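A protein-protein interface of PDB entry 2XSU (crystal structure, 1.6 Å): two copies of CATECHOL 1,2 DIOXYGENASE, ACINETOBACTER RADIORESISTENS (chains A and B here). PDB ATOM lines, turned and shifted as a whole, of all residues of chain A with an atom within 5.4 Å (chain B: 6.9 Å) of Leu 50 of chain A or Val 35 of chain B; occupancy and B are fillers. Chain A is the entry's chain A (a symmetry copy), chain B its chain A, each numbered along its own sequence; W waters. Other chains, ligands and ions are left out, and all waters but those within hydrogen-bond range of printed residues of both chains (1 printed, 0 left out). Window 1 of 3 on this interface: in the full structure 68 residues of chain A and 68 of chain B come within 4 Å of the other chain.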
ATOM      1  N   GLN A  45      -5.978 -13.903  22.868  1.00  0.00           N
ATOM      2  CA  GLN A  45      -6.210 -13.052  24.007  1.00  0.00           C
ATOM      3  C   GLN A  45      -4.958 -12.232  24.384  1.00  0.00           C
ATOM      4  O   GLN A  45      -5.064 -11.065  24.776  1.00  0.00           O
ATOM      5  CB  GLN A  45      -6.720 -13.869  25.187  1.00  0.00           C
ATOM      6  CG  GLN A  45      -7.095 -12.945  26.356  1.00  0.00           C
ATOM      7  CD  GLN A  45      -8.342 -12.129  26.102  1.00  0.00           C
ATOM      8  OE1 GLN A  45      -8.290 -10.896  26.048  1.00  0.00           O
ATOM      9  NE2 GLN A  45      -9.480 -12.809  25.967  1.00  0.00           N
ATOM     10  N   ALA A  46      -3.772 -12.834  24.257  1.00  0.00           N
ATOM     11  CA  ALA A  46      -2.538 -12.082  24.465  1.00  0.00           C
ATOM     12  C   ALA A  46      -2.370 -10.966  23.420  1.00  0.00           C
ATOM     13  O   ALA A  46      -1.920  -9.875  23.725  1.00  0.00           O
ATOM     14  CB  ALA A  46      -1.308 -13.038  24.464  1.00  0.00           C
ATOM     15  N   ILE A  47      -2.733 -11.266  22.167  1.00  0.00           N
ATOM     16  CA  ILE A  47      -2.689 -10.257  21.113  1.00  0.00           C
ATOM     17  C   ILE A  47      -3.603  -9.070  21.476  1.00  0.00           C
ATOM     18  O   ILE A  47      -3.207  -7.923  21.326  1.00  0.00           O
ATOM     19  CB  ILE A  47      -3.080 -10.871  19.746  1.00  0.00           C
ATOM     20  CG1 ILE A  47      -1.902 -11.706  19.232  1.00  0.00           C
ATOM     21  CG2 ILE A  47      -3.317  -9.776  18.676  1.00  0.00           C
ATOM     22  CD1 ILE A  47      -2.226 -12.707  18.118  1.00  0.00           C
ATOM     23  N   GLU A  48      -4.806  -9.356  21.973  1.00  0.00           N
ATOM     24  CA  GLU A  48      -5.712  -8.285  22.416  1.00  0.00           C
ATOM     25  C   GLU A  48      -5.131  -7.515  23.608  1.00  0.00           C
ATOM     26  O   GLU A  48      -5.059  -6.277  23.591  1.00  0.00           O
ATOM     27  CB  GLU A  48      -7.081  -8.825  22.796  1.00  0.00           C
ATOM     28  CG  GLU A  48      -7.848  -9.446  21.655  1.00  0.00           C
ATOM     29  CD  GLU A  48      -8.310  -8.420  20.615  1.00  0.00           C
ATOM     30  OE1 GLU A  48      -8.335  -7.198  20.899  1.00  0.00           O
ATOM     31  OE2 GLU A  48      -8.657  -8.864  19.503  1.00  0.00           O
ATOM     32  N   ASP A  49      -4.713  -8.253  24.637  1.00  0.00           N
ATOM     33  CA  ASP A  49      -4.303  -7.594  25.882  1.00  0.00           C
ATOM     34  C   ASP A  49      -3.079  -6.704  25.713  1.00  0.00           C
ATOM     35  O   ASP A  49      -2.982  -5.620  26.320  1.00  0.00           O
ATOM     36  CB  ASP A  49      -4.042  -8.602  27.003  1.00  0.00           C
ATOM     37  CG  ASP A  49      -5.316  -9.246  27.564  1.00  0.00           C
ATOM     38  OD1 ASP A  49      -6.449  -8.726  27.372  1.00  0.00           O
ATOM     39  OD2 ASP A  49      -5.199 -10.282  28.242  1.00  0.00           O
ATOM     40  N   LEU A  50      -2.117  -7.156  24.908  1.00  0.00           N
ATOM     41  CA  LEU A  50      -0.868  -6.435  24.698  1.00  0.00           C
ATOM     42  C   LEU A  50      -0.882  -5.569  23.420  1.00  0.00           C
ATOM     43  O   LEU A  50       0.136  -4.970  23.055  1.00  0.00           O
ATOM     44  CB  LEU A  50       0.308  -7.447  24.715  1.00  0.00           C
ATOM     45  CG  LEU A  50       0.867  -7.867  26.070  1.00  0.00           C
ATOM     46  CD1 LEU A  50      -0.144  -8.554  26.913  1.00  0.00           C
ATOM     47  CD2 LEU A  50       2.059  -8.792  25.867  1.00  0.00           C
ATOM     48  N   ASP A  51      -2.037  -5.573  22.732  1.00  0.00           N
ATOM     49  CA  ASP A  51      -2.238  -4.910  21.429  1.00  0.00           C
ATOM     50  C   ASP A  51      -1.078  -5.208  20.473  1.00  0.00           C
ATOM     51  O   ASP A  51      -0.376  -4.312  19.966  1.00  0.00           O
ATOM     52  CB  ASP A  51      -2.443  -3.403  21.631  1.00  0.00           C
ATOM     53  CG  ASP A  51      -2.949  -2.707  20.373  1.00  0.00           C
ATOM     54  OD1 ASP A  51      -3.577  -3.363  19.492  1.00  0.00           O
ATOM     55  OD2 ASP A  51      -2.732  -1.473  20.282  1.00  0.00           O
ATOM     56  N   ILE A  52      -0.840  -6.505  20.272  1.00  0.00           N
ATOM     57  CA  ILE A  52       0.237  -6.986  19.414  1.00  0.00           C
ATOM     58  C   ILE A  52      -0.146  -6.739  17.947  1.00  0.00           C
ATOM     59  O   ILE A  52      -1.211  -7.161  17.483  1.00  0.00           O
ATOM     60  CB  ILE A  52       0.581  -8.473  19.688  1.00  0.00           C
ATOM     61  CG1 ILE A  52       0.823  -8.671  21.201  1.00  0.00           C
ATOM     62  CG2 ILE A  52       1.818  -8.887  18.863  1.00  0.00           C
ATOM     63  CD1 ILE A  52       1.248 -10.139  21.580  1.00  0.00           C
ATOM     64  N   GLU B  30      12.349  -3.692  26.045  1.00  0.00           N
ATOM     65  CA  GLU B  30      11.229  -3.788  26.976  1.00  0.00           C
ATOM     66  C   GLU B  30      10.000  -4.489  26.372  1.00  0.00           C
ATOM     67  O   GLU B  30       9.304  -5.236  27.078  1.00  0.00           O
ATOM     68  CB  GLU B  30      10.873  -2.417  27.564  1.00  0.00           C
ATOM     69  CG  GLU B  30      12.048  -1.857  28.395  1.00  0.00           C
ATOM     70  CD  GLU B  30      11.697  -0.650  29.248  1.00  0.00           C
ATOM     71  OE1 GLU B  30      10.528  -0.531  29.687  1.00  0.00           O
ATOM     72  OE2 GLU B  30      12.614   0.176  29.492  1.00  0.00           O
ATOM     73  N   ARG B  31       9.742  -4.245  25.081  1.00  0.00           N
ATOM     74  CA  ARG B  31       8.581  -4.845  24.388  1.00  0.00           C
ATOM     75  C   ARG B  31       8.753  -6.365  24.247  1.00  0.00           C
ATOM     76  O   ARG B  31       7.818  -7.142  24.548  1.00  0.00           O
ATOM     77  CB  ARG B  31       8.360  -4.196  23.009  1.00  0.00           C
ATOM     78  CG  ARG B  31       7.158  -4.801  22.230  1.00  0.00           C
ATOM     79  CD  ARG B  31       5.848  -4.689  22.996  1.00  0.00           C
ATOM     80  NE  ARG B  31       4.707  -4.876  22.079  1.00  0.00           N
ATOM     81  CZ  ARG B  31       3.426  -4.909  22.424  1.00  0.00           C
ATOM     82  NH1 ARG B  31       3.030  -4.817  23.712  1.00  0.00           N
ATOM     83  NH2 ARG B  31       2.525  -5.036  21.442  1.00  0.00           N
ATOM     84  N   ILE B  32       9.952  -6.772  23.849  1.00  0.00           N
ATOM     85  CA  ILE B  32      10.232  -8.213  23.695  1.00  0.00           C
ATOM     86  C   ILE B  32      10.132  -8.888  25.070  1.00  0.00           C
ATOM     87  O   ILE B  32       9.514  -9.952  25.202  1.00  0.00           O
ATOM     88  CB  ILE B  32      11.576  -8.465  22.994  1.00  0.00           C
ATOM     89  CG1 ILE B  32      11.487  -8.037  21.519  1.00  0.00           C
ATOM     90  CG2 ILE B  32      11.957  -9.946  23.069  1.00  0.00           C
ATOM     91  CD1 ILE B  32      12.798  -8.043  20.769  1.00  0.00           C
ATOM     92  N   GLN B  33      10.716  -8.270  26.103  1.00  0.00           N
ATOM     93  CA  GLN B  33      10.580  -8.810  27.454  1.00  0.00           C
ATOM     94  C   GLN B  33       9.109  -8.984  27.871  1.00  0.00           C
ATOM     95  O   GLN B  33       8.704 -10.037  28.344  1.00  0.00           O
ATOM     96  CB  GLN B  33      11.361  -7.964  28.458  1.00  0.00           C
ATOM     97  CG  GLN B  33      11.371  -8.560  29.872  1.00  0.00           C
ATOM     98  CD  GLN B  33      11.910  -7.553  30.885  1.00  0.00           C
ATOM     99  OE1 GLN B  33      11.214  -6.597  31.232  1.00  0.00           O
ATOM    100  NE2 GLN B  33      13.149  -7.754  31.343  1.00  0.00           N
ATOM    101  N   GLN B  34       8.308  -7.935  27.686  1.00  0.00           N
ATOM    102  CA  GLN B  34       6.879  -7.969  27.999  1.00  0.00           C
ATOM    103  C   GLN B  34       6.149  -9.145  27.302  1.00  0.00           C
ATOM    104  O   GLN B  34       5.400  -9.881  27.935  1.00  0.00           O
ATOM    105  CB  GLN B  34       6.249  -6.633  27.543  1.00  0.00           C
ATOM    106  CG  GLN B  34       4.782  -6.538  27.838  1.00  0.00           C
ATOM    107  CD  GLN B  34       4.089  -5.378  27.118  1.00  0.00           C
ATOM    108  OE1 GLN B  34       4.597  -4.820  26.149  1.00  0.00           O
ATOM    109  NE2 GLN B  34       2.907  -5.033  27.601  1.00  0.00           N
ATOM    110  N   VAL B  35       6.363  -9.287  25.995  1.00  0.00           N
ATOM    111  CA  VAL B  35       5.681 -10.322  25.220  1.00  0.00           C
ATOM    112  C   VAL B  35       6.131 -11.739  25.636  1.00  0.00           C
ATOM    113  O   VAL B  35       5.281 -12.617  25.866  1.00  0.00           O
ATOM    114  CB  VAL B  35       5.840 -10.098  23.677  1.00  0.00           C
ATOM    115  CG1 VAL B  35       5.270 -11.319  22.888  1.00  0.00           C
ATOM    116  CG2 VAL B  35       5.220  -8.765  23.240  1.00  0.00           C
ATOM    117  N   VAL B  36       7.437 -11.940  25.807  1.00  0.00           N
ATOM    118  CA  VAL B  36       7.956 -13.237  26.251  1.00  0.00           C
ATOM    119  C   VAL B  36       7.395 -13.650  27.621  1.00  0.00           C
ATOM    120  O   VAL B  36       6.943 -14.799  27.807  1.00  0.00           O
ATOM    121  CB  VAL B  36       9.505 -13.236  26.227  1.00  0.00           C
ATOM    122  CG1 VAL B  36      10.073 -14.453  26.979  1.00  0.00           C
ATOM    123  CG2 VAL B  36       9.989 -13.138  24.762  1.00  0.00           C
ATOM    124  N   VAL B  37       7.395 -12.728  28.583  1.00  0.00           N
ATOM    125  CA  VAL B  37       6.880 -13.011  29.916  1.00  0.00           C
ATOM    126  C   VAL B  37       5.401 -13.418  29.862  1.00  0.00           C
ATOM    127  O   VAL B  37       4.976 -14.363  30.517  1.00  0.00           O
ATOM    128  CB  VAL B  37       7.134 -11.809  30.846  1.00  0.00           C
ATOM    129  CG1 VAL B  37       6.369 -11.951  32.151  1.00  0.00           C
ATOM    130  CG2 VAL B  37       8.620 -11.693  31.117  1.00  0.00           C
ATOM    131  N   ARG B  38       4.616 -12.700  29.069  1.00  0.00           N
ATOM    132  CA  ARG B  38       3.203 -13.024  28.922  1.00  0.00           C
ATOM    133  C   ARG B  38       2.979 -14.385  28.268  1.00  0.00           C
ATOM    134  O   ARG B  38       2.216 -15.203  28.796  1.00  0.00           O
ATOM    135  CB  ARG B  38       2.490 -11.901  28.144  1.00  0.00           C
ATOM    136  CG  ARG B  38       1.029 -12.236  27.725  1.00  0.00           C
ATOM    137  CD  ARG B  38       0.087 -12.507  28.912  1.00  0.00           C
ATOM    138  NE  ARG B  38      -1.253 -12.875  28.436  1.00  0.00           N
ATOM    139  CZ  ARG B  38      -2.285 -12.030  28.436  1.00  0.00           C
ATOM    140  NH1 ARG B  38      -2.145 -10.814  28.958  1.00  0.00           N
ATOM    141  NH2 ARG B  38      -3.464 -12.429  27.976  1.00  0.00           N
ATOM    142  N   LEU B  39       3.637 -14.628  27.136  1.00  0.00           N
ATOM    143  CA  LEU B  39       3.405 -15.881  26.411  1.00  0.00           C
ATOM    144  C   LEU B  39       3.909 -17.090  27.184  1.00  0.00           C
ATOM    145  O   LEU B  39       3.259 -18.134  27.156  1.00  0.00           O
ATOM    146  CB  LEU B  39       4.001 -15.851  24.995  1.00  0.00           C
ATOM    147  CG  LEU B  39       3.374 -14.797  24.073  1.00  0.00           C
ATOM    148  CD1 LEU B  39       4.120 -14.815  22.743  1.00  0.00           C
ATOM    149  CD2 LEU B  39       1.860 -15.003  23.882  1.00  0.00           C
ATOM    150  N   LEU B  40       5.044 -16.952  27.876  1.00  0.00           N
ATOM    151  CA  LEU B  40       5.554 -18.084  28.662  1.00  0.00           C
ATOM    152  C   LEU B  40       4.653 -18.390  29.845  1.00  0.00           C
ATOM    153  O   LEU B  40       4.372 -19.545  30.131  1.00  0.00           O
ATOM    154  CB  LEU B  40       6.967 -17.812  29.175  1.00  0.00           C
ATOM    155  CG  LEU B  40       8.102 -18.104  28.207  1.00  0.00           C
ATOM    156  CD1 LEU B  40       9.400 -17.485  28.763  1.00  0.00           C
ATOM    157  CD2 LEU B  40       8.222 -19.648  28.080  1.00  0.00           C
ATOM    158  N   GLY B  41       4.209 -17.344  30.546  1.00  0.00           N
ATOM    159  CA  GLY B  41       3.268 -17.549  31.645  1.00  0.00           C
ATOM    160  C   GLY B  41       1.989 -18.240  31.149  1.00  0.00           C
ATOM    161  O   GLY B  41       1.479 -19.165  31.780  1.00  0.00           O
ATOM    162  N   ARG B  89      -8.947  -7.635  13.673  1.00  0.00           N
ATOM    163  CA  ARG B  89      -8.447  -6.572  14.555  1.00  0.00           C
ATOM    164  C   ARG B  89      -8.208  -5.257  13.810  1.00  0.00           C
ATOM    165  O   ARG B  89      -8.573  -4.189  14.313  1.00  0.00           O
ATOM    166  CB  ARG B  89      -7.188  -7.020  15.293  1.00  0.00           C
ATOM    167  CG  ARG B  89      -7.502  -8.037  16.354  1.00  0.00           C
ATOM    168  CD  ARG B  89      -6.310  -8.208  17.318  1.00  0.00           C
ATOM    169  NE  ARG B  89      -6.435  -7.212  18.432  1.00  0.00           N
ATOM    170  CZ  ARG B  89      -5.540  -6.278  18.742  1.00  0.00           C
ATOM    171  NH1 ARG B  89      -4.391  -6.124  18.089  1.00  0.00           N
ATOM    172  NH2 ARG B  89      -5.799  -5.451  19.738  1.00  0.00           N
HETATM  173  O   HOH W   1      -3.309  -7.635  15.741  1.00  0.00           O
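No position is printed for both chains.
NH2 of Arg 89 of chain B is in salt-bridge range of OD1 of Asp 51 of chain A (3.1 Å). The guanidinium group (NE) of Arg 89 of chain B is in salt-bridge range of the side-chain carboxylate (OE2) of Glu 48 of chain A (3.0 Å). The backbone carbonyl oxygen (O) of Asp 51 of chain A is in hydrogen-bond range of the guanidinium group (NH2) of Arg 31 of chain B, at 3.3 Å. NH2 of Arg 31 of chain B is in hydrogen-bond range of O of Leu 50 of chain A. The backbone carbonyl oxygen of Ile 52 of chain A lies within hydrogen-bond range of the guanidinium group of Arg 89 of chain B (3.4 Å). The side-chain carboxylate (OD2) of Asp 49 of chain A is in salt-bridge range of the guanidinium group (NH2) of Arg 38 of chain B.
Printed residues of chain B within 4 Å of Glu 48 of chain A: Arg 89. Printed residues of chain B within 4 Å of Leu 50 of chain A: Arg 31 (2.9 Å), Gln 34 (3.8 Å), Val 35 (3.98 Å) and Arg 38 (3.6 Å). Printed residues of chain B within 4 Å of Asp 51 of chain A: Arg 31 (3.3 Å) and Arg 89 (3.1 Å). Of the printed residues of chain A, Arg 31 of chain B touches Leu 50, Asp 51 and Ile 52. Printed residues of chain A within 4 Å of Val 35 of chain B: Leu 50. Val 37 of chain B touches none of the printed residues of chain A. The nearest printed residue of chain B that does not touch Leu 50 of chain A is Arg 89 of chain B (6.1 Å). The nearest printed residue of chain B that does not touch Asp 51 of chain A is Gln 34 of chain B (7.0 Å).
Water W1 bridges the backbone carbonyl oxygen (O) of Ile 52 of chain A (2.8 Å) and the guanidinium group (NH1) of Arg 89 of chain B (3.0 Å).
O of Gln 45 of chain A touches NH2 of Arg 38 of chain B, at 3.8 Å. CA of Ala 46 of chain A touches NH2 of Arg 38 of chain B, at 3.6 Å. Leu 39 of chain B touches Ala 46 of chain A. Arg 89 of chain B touches Ile 47 of chain A. CG of Leu 50 of chain A touches NE2 of Gln 34 of chain B (3.8 Å). Leu 50 of chain A touches Val 35 of chain B. Leu 50 of chain A touches Arg 38 of chain B. Ile 52 of chain A touches Arg 31 of chain B.
Hydrophobic or aromatic side chains of chain A within 4 Å of the printed part of chain B: Ala 46, Ile 47 and Leu 50. Along chain A the printed residues that touch a printed residue of chain B span positions 45 to 52. Of the 13 printed residues of chain B, 6 touch a printed residue of chain A. Printed residues of chain B that touch a printed residue of chain A: Arg 31, Gln 34, Val 35, Arg 38, Leu 39 and Arg 89. Hydrophobic or aromatic side chains of chain B within 4 Å of the printed part of chain A: Leu 39. Among the printed residues, 14 pairs touch across the chains. Among the printed residues, Asp or Glu carboxylates within 4 Å of a Lys or Arg side-chain nitrogen of the other chain: Glu 48 of chain A with Arg 89 of chain B, Asp 49 of chain A with Arg 38 of chain B and Asp 51 of chain A with Arg 89 of chain B.
The side-chain amide oxygen of Gln 34 of chain B is in hydrogen-bond range of the guanidinium group of Arg 31 of chain B (2.9 Å). The side-chain carboxylate (OD1) of Asp 49 of chain A sits close to the side-chain amide oxygen (OE1) of Gln 45 of chain A, 3.1 Å away. O of Ile 47 of chain A is in hydrogen-bond range of N of Ile 52 of chain A, at 3.0 Å.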
